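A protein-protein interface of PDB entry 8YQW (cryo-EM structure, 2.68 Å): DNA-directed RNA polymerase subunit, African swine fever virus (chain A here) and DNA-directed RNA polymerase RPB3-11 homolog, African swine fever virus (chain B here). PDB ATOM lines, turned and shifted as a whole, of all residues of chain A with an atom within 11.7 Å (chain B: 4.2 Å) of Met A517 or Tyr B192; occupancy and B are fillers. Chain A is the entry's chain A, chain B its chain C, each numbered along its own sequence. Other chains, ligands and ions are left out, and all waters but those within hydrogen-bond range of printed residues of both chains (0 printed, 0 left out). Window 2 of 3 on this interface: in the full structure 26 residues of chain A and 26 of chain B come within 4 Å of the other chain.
The backbone carbonyl oxygen (O) of Tyr B205 sits close to the side-chain sulfur (SD) of Met A517.
N of Tyr B192 is in hydrogen-bond range of O of Gly B204, at 2.6 Å.
Among the printed residues, merely in contact across the chains: Pro A516 with Leu B202, Met A517 with Tyr B192, Met A517 with Leu B202 and Met A517 with Lys B206.
Printed residues of chain B within 4 Å of Pro A516: Leu B202 (3.7 Å). Met A517 touches just these residues of chain B: Tyr B192, Leu B202, Tyr B205 and Lys B206. Printed residues of chain A within 4 Å of Tyr B192: Met A517. No residue of chain A comes within 4 Å of Pro B193. No residue of chain A comes within 4 Å of Thr B194. Printed residues of chain A within 4 Å of Leu B202: Pro A516 and Met A517. No residue of chain A comes within 4 Å of Gly B204. Printed residues of chain A within 4 Å of Tyr B205: Met A517. Gln B207 touches none of the printed residues of chain A. The nearest printed residue of chain B that does not touch Pro A516 is Tyr B192 (5.5 Å).
Of the 22 printed residues of chain A, 2 touch a printed residue of chain B. Hydrophobic or aromatic side chains of chain A that line the printed part of chain B: Pro A516 and Met A517.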
ATOM      1  N   LEU A 509     -15.452   7.169   1.533  1.00  0.00           N
ATOM      2  CA  LEU A 509     -15.121   5.769   1.286  1.00  0.00           C
ATOM      3  C   LEU A 509     -15.573   5.328  -0.099  1.00  0.00           C
ATOM      4  O   LEU A 509     -14.889   4.536  -0.758  1.00  0.00           O
ATOM      5  CB  LEU A 509     -15.751   4.883   2.360  1.00  0.00           C
ATOM      6  CG  LEU A 509     -15.282   5.078   3.801  1.00  0.00           C
ATOM      7  CD1 LEU A 509     -16.217   4.374   4.761  1.00  0.00           C
ATOM      8  CD2 LEU A 509     -13.864   4.582   3.976  1.00  0.00           C
ATOM      9  N   ARG A 512     -13.328   7.161  -2.722  1.00  0.00           N
ATOM     10  CA  ARG A 512     -11.909   6.929  -2.501  1.00  0.00           C
ATOM     11  C   ARG A 512     -11.312   6.121  -3.647  1.00  0.00           C
ATOM     12  O   ARG A 512     -11.953   5.221  -4.192  1.00  0.00           O
ATOM     13  CB  ARG A 512     -11.732   6.201  -1.171  1.00  0.00           C
ATOM     14  CG  ARG A 512     -10.332   6.070  -0.658  1.00  0.00           C
ATOM     15  CD  ARG A 512     -10.369   5.374   0.687  1.00  0.00           C
ATOM     16  NE  ARG A 512     -11.388   4.332   0.729  1.00  0.00           N
ATOM     17  CZ  ARG A 512     -11.437   3.366   1.634  1.00  0.00           C
ATOM     18  NH1 ARG A 512     -10.529   3.270   2.592  1.00  0.00           N
ATOM     19  NH2 ARG A 512     -12.422   2.474   1.581  1.00  0.00           N
ATOM     20  N   THR A 513     -10.080   6.460  -4.027  1.00  0.00           N
ATOM     21  CA  THR A 513      -9.463   5.817  -5.185  1.00  0.00           C
ATOM     22  C   THR A 513      -9.058   4.382  -4.875  1.00  0.00           C
ATOM     23  O   THR A 513      -9.326   3.466  -5.661  1.00  0.00           O
ATOM     24  CB  THR A 513      -8.251   6.620  -5.656  1.00  0.00           C
ATOM     25  OG1 THR A 513      -8.674   7.915  -6.094  1.00  0.00           O
ATOM     26  CG2 THR A 513      -7.563   5.913  -6.805  1.00  0.00           C
ATOM     27  N   ASN A 514      -8.411   4.167  -3.734  1.00  0.00           N
ATOM     28  CA  ASN A 514      -7.893   2.861  -3.358  1.00  0.00           C
ATOM     29  C   ASN A 514      -8.467   2.432  -2.017  1.00  0.00           C
ATOM     30  O   ASN A 514      -8.913   3.256  -1.218  1.00  0.00           O
ATOM     31  CB  ASN A 514      -6.363   2.859  -3.281  1.00  0.00           C
ATOM     32  CG  ASN A 514      -5.710   2.913  -4.644  1.00  0.00           C
ATOM     33  OD1 ASN A 514      -4.982   3.852  -4.958  1.00  0.00           O
ATOM     34  ND2 ASN A 514      -5.966   1.902  -5.462  1.00  0.00           N
ATOM     35  N   THR A 515      -8.445   1.136  -1.789  1.00  0.00           N
ATOM     36  CA  THR A 515      -8.935   0.415  -0.631  1.00  0.00           C
ATOM     37  C   THR A 515      -7.842  -0.521  -0.117  1.00  0.00           C
ATOM     38  O   THR A 515      -6.971  -0.932  -0.889  1.00  0.00           O
ATOM     39  CB  THR A 515     -10.190  -0.375  -1.031  1.00  0.00           C
ATOM     40  OG1 THR A 515     -11.226   0.543  -1.395  1.00  0.00           O
ATOM     41  CG2 THR A 515     -10.705  -1.273   0.077  1.00  0.00           C
ATOM     42  N   PRO A 516      -7.821  -0.847   1.181  1.00  0.00           N
ATOM     43  CA  PRO A 516      -6.899  -1.892   1.655  1.00  0.00           C
ATOM     44  C   PRO A 516      -6.983  -3.194   0.869  1.00  0.00           C
ATOM     45  O   PRO A 516      -6.061  -4.013   0.970  1.00  0.00           O
ATOM     46  CB  PRO A 516      -7.325  -2.093   3.112  1.00  0.00           C
ATOM     47  CG  PRO A 516      -7.832  -0.764   3.520  1.00  0.00           C
ATOM     48  CD  PRO A 516      -8.445  -0.125   2.305  1.00  0.00           C
ATOM     49  N   MET A 517      -8.045  -3.408   0.094  1.00  0.00           N
ATOM     50  CA  MET A 517      -8.190  -4.575  -0.766  1.00  0.00           C
ATOM     51  C   MET A 517      -7.712  -4.306  -2.187  1.00  0.00           C
ATOM     52  O   MET A 517      -7.912  -5.143  -3.073  1.00  0.00           O
ATOM     53  CB  MET A 517      -9.646  -5.042  -0.782  1.00  0.00           C
ATOM     54  CG  MET A 517     -10.076  -5.806   0.456  1.00  0.00           C
ATOM     55  SD  MET A 517      -9.369  -7.461   0.534  1.00  0.00           S
ATOM     56  CE  MET A 517      -8.088  -7.216   1.756  1.00  0.00           C
ATOM     57  N   GLY A 518      -7.089  -3.156  -2.424  1.00  0.00           N
ATOM     58  CA  GLY A 518      -6.637  -2.802  -3.754  1.00  0.00           C
ATOM     59  C   GLY A 518      -7.388  -1.627  -4.344  1.00  0.00           C
ATOM     60  O   GLY A 518      -7.551  -0.595  -3.689  1.00  0.00           O
ATOM     61  N   LYS A 519      -7.842  -1.767  -5.584  1.00  0.00           N
ATOM     62  CA  LYS A 519      -8.601  -0.706  -6.224  1.00  0.00           C
ATOM     63  C   LYS A 519     -10.040  -0.697  -5.720  1.00  0.00           C
ATOM     64  O   LYS A 519     -10.636  -1.740  -5.446  1.00  0.00           O
ATOM     65  CB  LYS A 519      -8.574  -0.873  -7.740  1.00  0.00           C
ATOM     66  CG  LYS A 519      -9.095   0.326  -8.499  1.00  0.00           C
ATOM     67  CD  LYS A 519      -8.856   0.181  -9.986  1.00  0.00           C
ATOM     68  CE  LYS A 519      -7.370   0.225 -10.292  1.00  0.00           C
ATOM     69  NZ  LYS A 519      -6.773   1.526  -9.885  1.00  0.00           N
ATOM     70  N   ASN A 520     -10.596   0.508  -5.596  1.00  0.00           N
ATOM     71  CA  ASN A 520     -11.942   0.701  -5.062  1.00  0.00           C
ATOM     72  C   ASN A 520     -12.947   0.546  -6.199  1.00  0.00           C
ATOM     73  O   ASN A 520     -13.462   1.516  -6.758  1.00  0.00           O
ATOM     74  CB  ASN A 520     -12.053   2.060  -4.388  1.00  0.00           C
ATOM     75  CG  ASN A 520     -13.255   2.170  -3.487  1.00  0.00           C
ATOM     76  OD1 ASN A 520     -14.008   1.214  -3.318  1.00  0.00           O
ATOM     77  ND2 ASN A 520     -13.443   3.341  -2.896  1.00  0.00           N
ATOM     78  N   VAL A 521     -13.228  -0.711  -6.543  1.00  0.00           N
ATOM     79  CA  VAL A 521     -14.170  -1.043  -7.600  1.00  0.00           C
ATOM     80  C   VAL A 521     -15.166  -2.068  -7.076  1.00  0.00           C
ATOM     81  O   VAL A 521     -14.926  -2.754  -6.082  1.00  0.00           O
ATOM     82  CB  VAL A 521     -13.471  -1.579  -8.868  1.00  0.00           C
ATOM     83  CG1 VAL A 521     -12.665  -0.483  -9.536  1.00  0.00           C
ATOM     84  CG2 VAL A 521     -12.587  -2.765  -8.528  1.00  0.00           C
ATOM     85  N   MET A 522     -16.299  -2.158  -7.764  1.00  0.00           N
ATOM     86  CA  MET A 522     -17.349  -3.109  -7.438  1.00  0.00           C
ATOM     87  C   MET A 522     -17.921  -3.666  -8.730  1.00  0.00           C
ATOM     88  O   MET A 522     -17.897  -3.004  -9.769  1.00  0.00           O
ATOM     89  CB  MET A 522     -18.452  -2.457  -6.599  1.00  0.00           C
ATOM     90  CG  MET A 522     -19.213  -1.368  -7.322  1.00  0.00           C
ATOM     91  SD  MET A 522     -20.051  -0.234  -6.203  1.00  0.00           S
ATOM     92  CE  MET A 522     -18.708   0.870  -5.784  1.00  0.00           C
ATOM     93  N   LEU A 549     -16.185  -4.259 -13.625  1.00  0.00           N
ATOM     94  CA  LEU A 549     -15.915  -3.567 -12.374  1.00  0.00           C
ATOM     95  C   LEU A 549     -16.147  -2.073 -12.549  1.00  0.00           C
ATOM     96  O   LEU A 549     -15.646  -1.468 -13.503  1.00  0.00           O
ATOM     97  CB  LEU A 549     -14.484  -3.833 -11.904  1.00  0.00           C
ATOM     98  CG  LEU A 549     -14.137  -5.304 -11.674  1.00  0.00           C
ATOM     99  CD1 LEU A 549     -12.640  -5.489 -11.517  1.00  0.00           C
ATOM    100  CD2 LEU A 549     -14.875  -5.846 -10.464  1.00  0.00           C
ATOM    101  N   TYR A 643     -22.962   1.951   0.176  1.00  0.00           N
ATOM    102  CA  TYR A 643     -21.577   1.518   0.029  1.00  0.00           C
ATOM    103  C   TYR A 643     -21.047   0.951   1.337  1.00  0.00           C
ATOM    104  O   TYR A 643     -20.457  -0.134   1.363  1.00  0.00           O
ATOM    105  CB  TYR A 643     -20.707   2.681  -0.445  1.00  0.00           C
ATOM    106  CG  TYR A 643     -19.268   2.292  -0.687  1.00  0.00           C
ATOM    107  CD1 TYR A 643     -18.862   1.799  -1.913  1.00  0.00           C
ATOM    108  CD2 TYR A 643     -18.317   2.414   0.314  1.00  0.00           C
ATOM    109  CE1 TYR A 643     -17.558   1.438  -2.137  1.00  0.00           C
ATOM    110  CE2 TYR A 643     -17.010   2.054   0.097  1.00  0.00           C
ATOM    111  CZ  TYR A 643     -16.636   1.568  -1.131  1.00  0.00           C
ATOM    112  OH  TYR A 643     -15.332   1.208  -1.355  1.00  0.00           O
ATOM    113  N   ASN A 646     -21.717  -2.812   2.902  1.00  0.00           N
ATOM    114  CA  ASN A 646     -20.807  -3.950   2.912  1.00  0.00           C
ATOM    115  C   ASN A 646     -19.344  -3.532   2.864  1.00  0.00           C
ATOM    116  O   ASN A 646     -18.478  -4.390   2.661  1.00  0.00           O
ATOM    117  CB  ASN A 646     -21.105  -4.908   1.759  1.00  0.00           C
ATOM    118  CG  ASN A 646     -21.209  -4.205   0.439  1.00  0.00           C
ATOM    119  OD1 ASN A 646     -21.124  -2.984   0.373  1.00  0.00           O
ATOM    120  ND2 ASN A 646     -21.389  -4.968  -0.627  1.00  0.00           N
ATOM    121  N   ALA A 647     -19.038  -2.249   3.032  1.00  0.00           N
ATOM    122  CA  ALA A 647     -17.667  -1.823   3.269  1.00  0.00           C
ATOM    123  C   ALA A 647     -17.338  -1.832   4.752  1.00  0.00           C
ATOM    124  O   ALA A 647     -16.213  -2.163   5.137  1.00  0.00           O
ATOM    125  CB  ALA A 647     -17.432  -0.428   2.689  1.00  0.00           C
ATOM    126  N   GLY A 648     -18.305  -1.477   5.588  1.00  0.00           N
ATOM    127  CA  GLY A 648     -18.114  -1.472   7.021  1.00  0.00           C
ATOM    128  C   GLY A 648     -17.347  -0.264   7.508  1.00  0.00           C
ATOM    129  O   GLY A 648     -16.428   0.212   6.838  1.00  0.00           O
ATOM    130  N   ASN A 724      -3.036   3.865  10.788  1.00  0.00           N
ATOM    131  CA  ASN A 724      -3.106   3.657   9.350  1.00  0.00           C
ATOM    132  C   ASN A 724      -4.275   4.464   8.809  1.00  0.00           C
ATOM    133  O   ASN A 724      -5.432   4.138   9.110  1.00  0.00           O
ATOM    134  CB  ASN A 724      -3.278   2.174   9.023  1.00  0.00           C
ATOM    135  CG  ASN A 724      -3.033   1.867   7.561  1.00  0.00           C
ATOM    136  OD1 ASN A 724      -2.785   2.762   6.758  1.00  0.00           O
ATOM    137  ND2 ASN A 724      -3.094   0.591   7.210  1.00  0.00           N
ATOM    138  N   PRO A 725      -4.034   5.523   8.034  1.00  0.00           N
ATOM    139  CA  PRO A 725      -5.157   6.342   7.547  1.00  0.00           C
ATOM    140  C   PRO A 725      -6.151   5.574   6.695  1.00  0.00           C
ATOM    141  O   PRO A 725      -7.328   5.948   6.647  1.00  0.00           O
ATOM    142  CB  PRO A 725      -4.455   7.444   6.744  1.00  0.00           C
ATOM    143  CG  PRO A 725      -3.076   7.495   7.300  1.00  0.00           C
ATOM    144  CD  PRO A 725      -2.734   6.082   7.636  1.00  0.00           C
ATOM    145  N   GLU A 726      -5.716   4.512   6.016  1.00  0.00           N
ATOM    146  CA  GLU A 726      -6.631   3.729   5.197  1.00  0.00           C
ATOM    147  C   GLU A 726      -7.646   2.954   6.024  1.00  0.00           C
ATOM    148  O   GLU A 726      -8.761   2.720   5.547  1.00  0.00           O
ATOM    149  CB  GLU A 726      -5.854   2.754   4.314  1.00  0.00           C
ATOM    150  CG  GLU A 726      -5.016   3.414   3.248  1.00  0.00           C
ATOM    151  CD  GLU A 726      -4.386   2.406   2.312  1.00  0.00           C
ATOM    152  OE1 GLU A 726      -4.520   1.192   2.573  1.00  0.00           O
ATOM    153  OE2 GLU A 726      -3.766   2.825   1.313  1.00  0.00           O
ATOM    154  N   THR A 727      -7.294   2.546   7.240  1.00  0.00           N
ATOM    155  CA  THR A 727      -8.163   1.692   8.031  1.00  0.00           C
ATOM    156  C   THR A 727      -8.627   2.304   9.343  1.00  0.00           C
ATOM    157  O   THR A 727      -9.616   1.818   9.901  1.00  0.00           O
ATOM    158  CB  THR A 727      -7.471   0.356   8.338  1.00  0.00           C
ATOM    159  OG1 THR A 727      -6.297   0.592   9.121  1.00  0.00           O
ATOM    160  CG2 THR A 727      -7.078  -0.347   7.057  1.00  0.00           C
ATOM    161  N   GLN A 732     -10.347   8.721  10.182  1.00  0.00           N
ATOM    162  CA  GLN A 732     -11.163   9.035   9.015  1.00  0.00           C
ATOM    163  C   GLN A 732     -12.367   9.891   9.379  1.00  0.00           C
ATOM    164  O   GLN A 732     -12.820  10.696   8.560  1.00  0.00           O
ATOM    165  CB  GLN A 732     -11.618   7.750   8.331  1.00  0.00           C
ATOM    166  CG  GLN A 732     -10.548   7.080   7.497  1.00  0.00           C
ATOM    167  CD  GLN A 732     -10.945   5.691   7.060  1.00  0.00           C
ATOM    168  OE1 GLN A 732     -11.934   5.139   7.535  1.00  0.00           O
ATOM    169  NE2 GLN A 732     -10.179   5.118   6.147  1.00  0.00           N
ATOM    170  N   GLN B 191      -8.110 -16.567   2.935  1.00  0.00           N
ATOM    171  CA  GLN B 191      -8.137 -15.697   4.099  1.00  0.00           C
ATOM    172  C   GLN B 191      -6.726 -15.310   4.513  1.00  0.00           C
ATOM    173  O   GLN B 191      -5.770 -16.061   4.311  1.00  0.00           O
ATOM    174  CB  GLN B 191      -8.845 -16.357   5.290  1.00  0.00           C
ATOM    175  CG  GLN B 191     -10.272 -16.778   5.018  1.00  0.00           C
ATOM    176  CD  GLN B 191     -11.078 -16.936   6.289  1.00  0.00           C
ATOM    177  OE1 GLN B 191     -10.700 -16.427   7.341  1.00  0.00           O
ATOM    178  NE2 GLN B 191     -12.192 -17.652   6.200  1.00  0.00           N
ATOM    179  N   TYR B 192      -6.614 -14.119   5.090  1.00  0.00           N
ATOM    180  CA  TYR B 192      -5.384 -13.662   5.708  1.00  0.00           C
ATOM    181  C   TYR B 192      -5.250 -14.237   7.111  1.00  0.00           C
ATOM    182  O   TYR B 192      -6.241 -14.632   7.729  1.00  0.00           O
ATOM    183  CB  TYR B 192      -5.366 -12.141   5.796  1.00  0.00           C
ATOM    184  CG  TYR B 192      -5.254 -11.420   4.479  1.00  0.00           C
ATOM    185  CD1 TYR B 192      -4.168 -11.624   3.642  1.00  0.00           C
ATOM    186  CD2 TYR B 192      -6.225 -10.516   4.082  1.00  0.00           C
ATOM    187  CE1 TYR B 192      -4.062 -10.957   2.441  1.00  0.00           C
ATOM    188  CE2 TYR B 192      -6.127  -9.848   2.887  1.00  0.00           C
ATOM    189  CZ  TYR B 192      -5.045 -10.068   2.069  1.00  0.00           C
ATOM    190  OH  TYR B 192      -4.950  -9.398   0.872  1.00  0.00           O
ATOM    191  N   PRO B 193      -4.032 -14.298   7.640  1.00  0.00           N
ATOM    192  CA  PRO B 193      -3.856 -14.469   9.088  1.00  0.00           C
ATOM    193  C   PRO B 193      -4.090 -13.141   9.790  1.00  0.00           C
ATOM    194  O   PRO B 193      -3.252 -12.236   9.737  1.00  0.00           O
ATOM    195  CB  PRO B 193      -2.398 -14.936   9.210  1.00  0.00           C
ATOM    196  CG  PRO B 193      -1.949 -15.252   7.806  1.00  0.00           C
ATOM    197  CD  PRO B 193      -2.751 -14.371   6.923  1.00  0.00           C
ATOM    198  N   THR B 194      -5.238 -13.017  10.451  1.00  0.00           N
ATOM    199  CA  THR B 194      -5.635 -11.742  11.035  1.00  0.00           C
ATOM    200  C   THR B 194      -5.002 -11.489  12.395  1.00  0.00           C
ATOM    201  O   THR B 194      -5.259 -10.439  12.993  1.00  0.00           O
ATOM    202  CB  THR B 194      -7.158 -11.663  11.152  1.00  0.00           C
ATOM    203  OG1 THR B 194      -7.666 -12.897  11.672  1.00  0.00           O
ATOM    204  CG2 THR B 194      -7.778 -11.394   9.792  1.00  0.00           C
ATOM    205  N   TYR B 199      -3.138  -6.856   9.402  1.00  0.00           N
ATOM    206  CA  TYR B 199      -4.375  -7.372   8.841  1.00  0.00           C
ATOM    207  C   TYR B 199      -5.534  -7.370   9.826  1.00  0.00           C
ATOM    208  O   TYR B 199      -6.637  -7.779   9.450  1.00  0.00           O
ATOM    209  CB  TYR B 199      -4.174  -8.806   8.331  1.00  0.00           C
ATOM    210  CG  TYR B 199      -3.271  -8.922   7.129  1.00  0.00           C
ATOM    211  CD1 TYR B 199      -3.407  -8.067   6.049  1.00  0.00           C
ATOM    212  CD2 TYR B 199      -2.284  -9.893   7.074  1.00  0.00           C
ATOM    213  CE1 TYR B 199      -2.585  -8.175   4.951  1.00  0.00           C
ATOM    214  CE2 TYR B 199      -1.456 -10.009   5.982  1.00  0.00           C
ATOM    215  CZ  TYR B 199      -1.611  -9.147   4.922  1.00  0.00           C
ATOM    216  OH  TYR B 199      -0.787  -9.259   3.826  1.00  0.00           O
ATOM    217  N   LEU B 202      -8.939  -5.626   8.931  1.00  0.00           N
ATOM    218  CA  LEU B 202      -9.693  -6.146   7.803  1.00  0.00           C
ATOM    219  C   LEU B 202     -10.474  -7.386   8.221  1.00  0.00           C
ATOM    220  O   LEU B 202     -10.204  -7.999   9.255  1.00  0.00           O
ATOM    221  CB  LEU B 202      -8.761  -6.479   6.637  1.00  0.00           C
ATOM    222  CG  LEU B 202      -7.634  -5.485   6.353  1.00  0.00           C
ATOM    223  CD1 LEU B 202      -6.819  -5.929   5.152  1.00  0.00           C
ATOM    224  CD2 LEU B 202      -8.186  -4.089   6.136  1.00  0.00           C
ATOM    225  N   GLY B 204     -10.549 -10.327   6.712  1.00  0.00           N
ATOM    226  CA  GLY B 204      -9.720 -11.511   6.618  1.00  0.00           C
ATOM    227  C   GLY B 204      -9.748 -12.144   5.246  1.00  0.00           C
ATOM    228  O   GLY B 204      -8.757 -12.731   4.809  1.00  0.00           O
ATOM    229  N   TYR B 205     -10.877 -12.029   4.555  1.00  0.00           N
ATOM    230  CA  TYR B 205     -10.985 -12.568   3.208  1.00  0.00           C
ATOM    231  C   TYR B 205     -10.104 -11.780   2.250  1.00  0.00           C
ATOM    232  O   TYR B 205     -10.006 -10.554   2.336  1.00  0.00           O
ATOM    233  CB  TYR B 205     -12.438 -12.535   2.740  1.00  0.00           C
ATOM    234  CG  TYR B 205     -13.321 -13.554   3.418  1.00  0.00           C
ATOM    235  CD1 TYR B 205     -13.139 -14.910   3.202  1.00  0.00           C
ATOM    236  CD2 TYR B 205     -14.335 -13.161   4.274  1.00  0.00           C
ATOM    237  CE1 TYR B 205     -13.941 -15.844   3.818  1.00  0.00           C
ATOM    238  CE2 TYR B 205     -15.143 -14.087   4.893  1.00  0.00           C
ATOM    239  CZ  TYR B 205     -14.940 -15.427   4.663  1.00  0.00           C
ATOM    240  OH  TYR B 205     -15.741 -16.356   5.279  1.00  0.00           O
ATOM    241  N   LYS B 206      -9.463 -12.493   1.328  1.00  0.00           N
ATOM    242  CA  LYS B 206      -8.539 -11.870   0.392  1.00  0.00           C
ATOM    243  C   LYS B 206      -9.238 -11.216  -0.791  1.00  0.00           C
ATOM    244  O   LYS B 206      -8.569 -10.568  -1.600  1.00  0.00           O
ATOM    245  CB  LYS B 206      -7.527 -12.899  -0.109  1.00  0.00           C
ATOM    246  CG  LYS B 206      -6.436 -13.215   0.889  1.00  0.00           C
ATOM    247  CD  LYS B 206      -5.432 -14.187   0.311  1.00  0.00           C
ATOM    248  CE  LYS B 206      -4.392 -14.570   1.341  1.00  0.00           C
ATOM    249  NZ  LYS B 206      -3.449 -15.595   0.820  1.00  0.00           N
ATOM    250  N   GLN B 207     -10.553 -11.368  -0.914  1.00  0.00           N
ATOM    251  CA  GLN B 207     -11.332 -10.684  -1.932  1.00  0.00           C
ATOM    252  C   GLN B 207     -12.305  -9.728  -1.260  1.00  0.00           C
ATOM    253  O   GLN B 207     -12.731  -9.948  -0.125  1.00  0.00           O
ATOM    254  CB  GLN B 207     -12.104 -11.671  -2.811  1.00  0.00           C
ATOM    255  CG  GLN B 207     -11.247 -12.743  -3.451  1.00  0.00           C
ATOM    256  CD  GLN B 207     -12.071 -13.763  -4.205  1.00  0.00           C
ATOM    257  OE1 GLN B 207     -13.278 -13.605  -4.362  1.00  0.00           O
ATOM    258  NE2 GLN B 207     -11.421 -14.822  -4.670  1.00  0.00           N
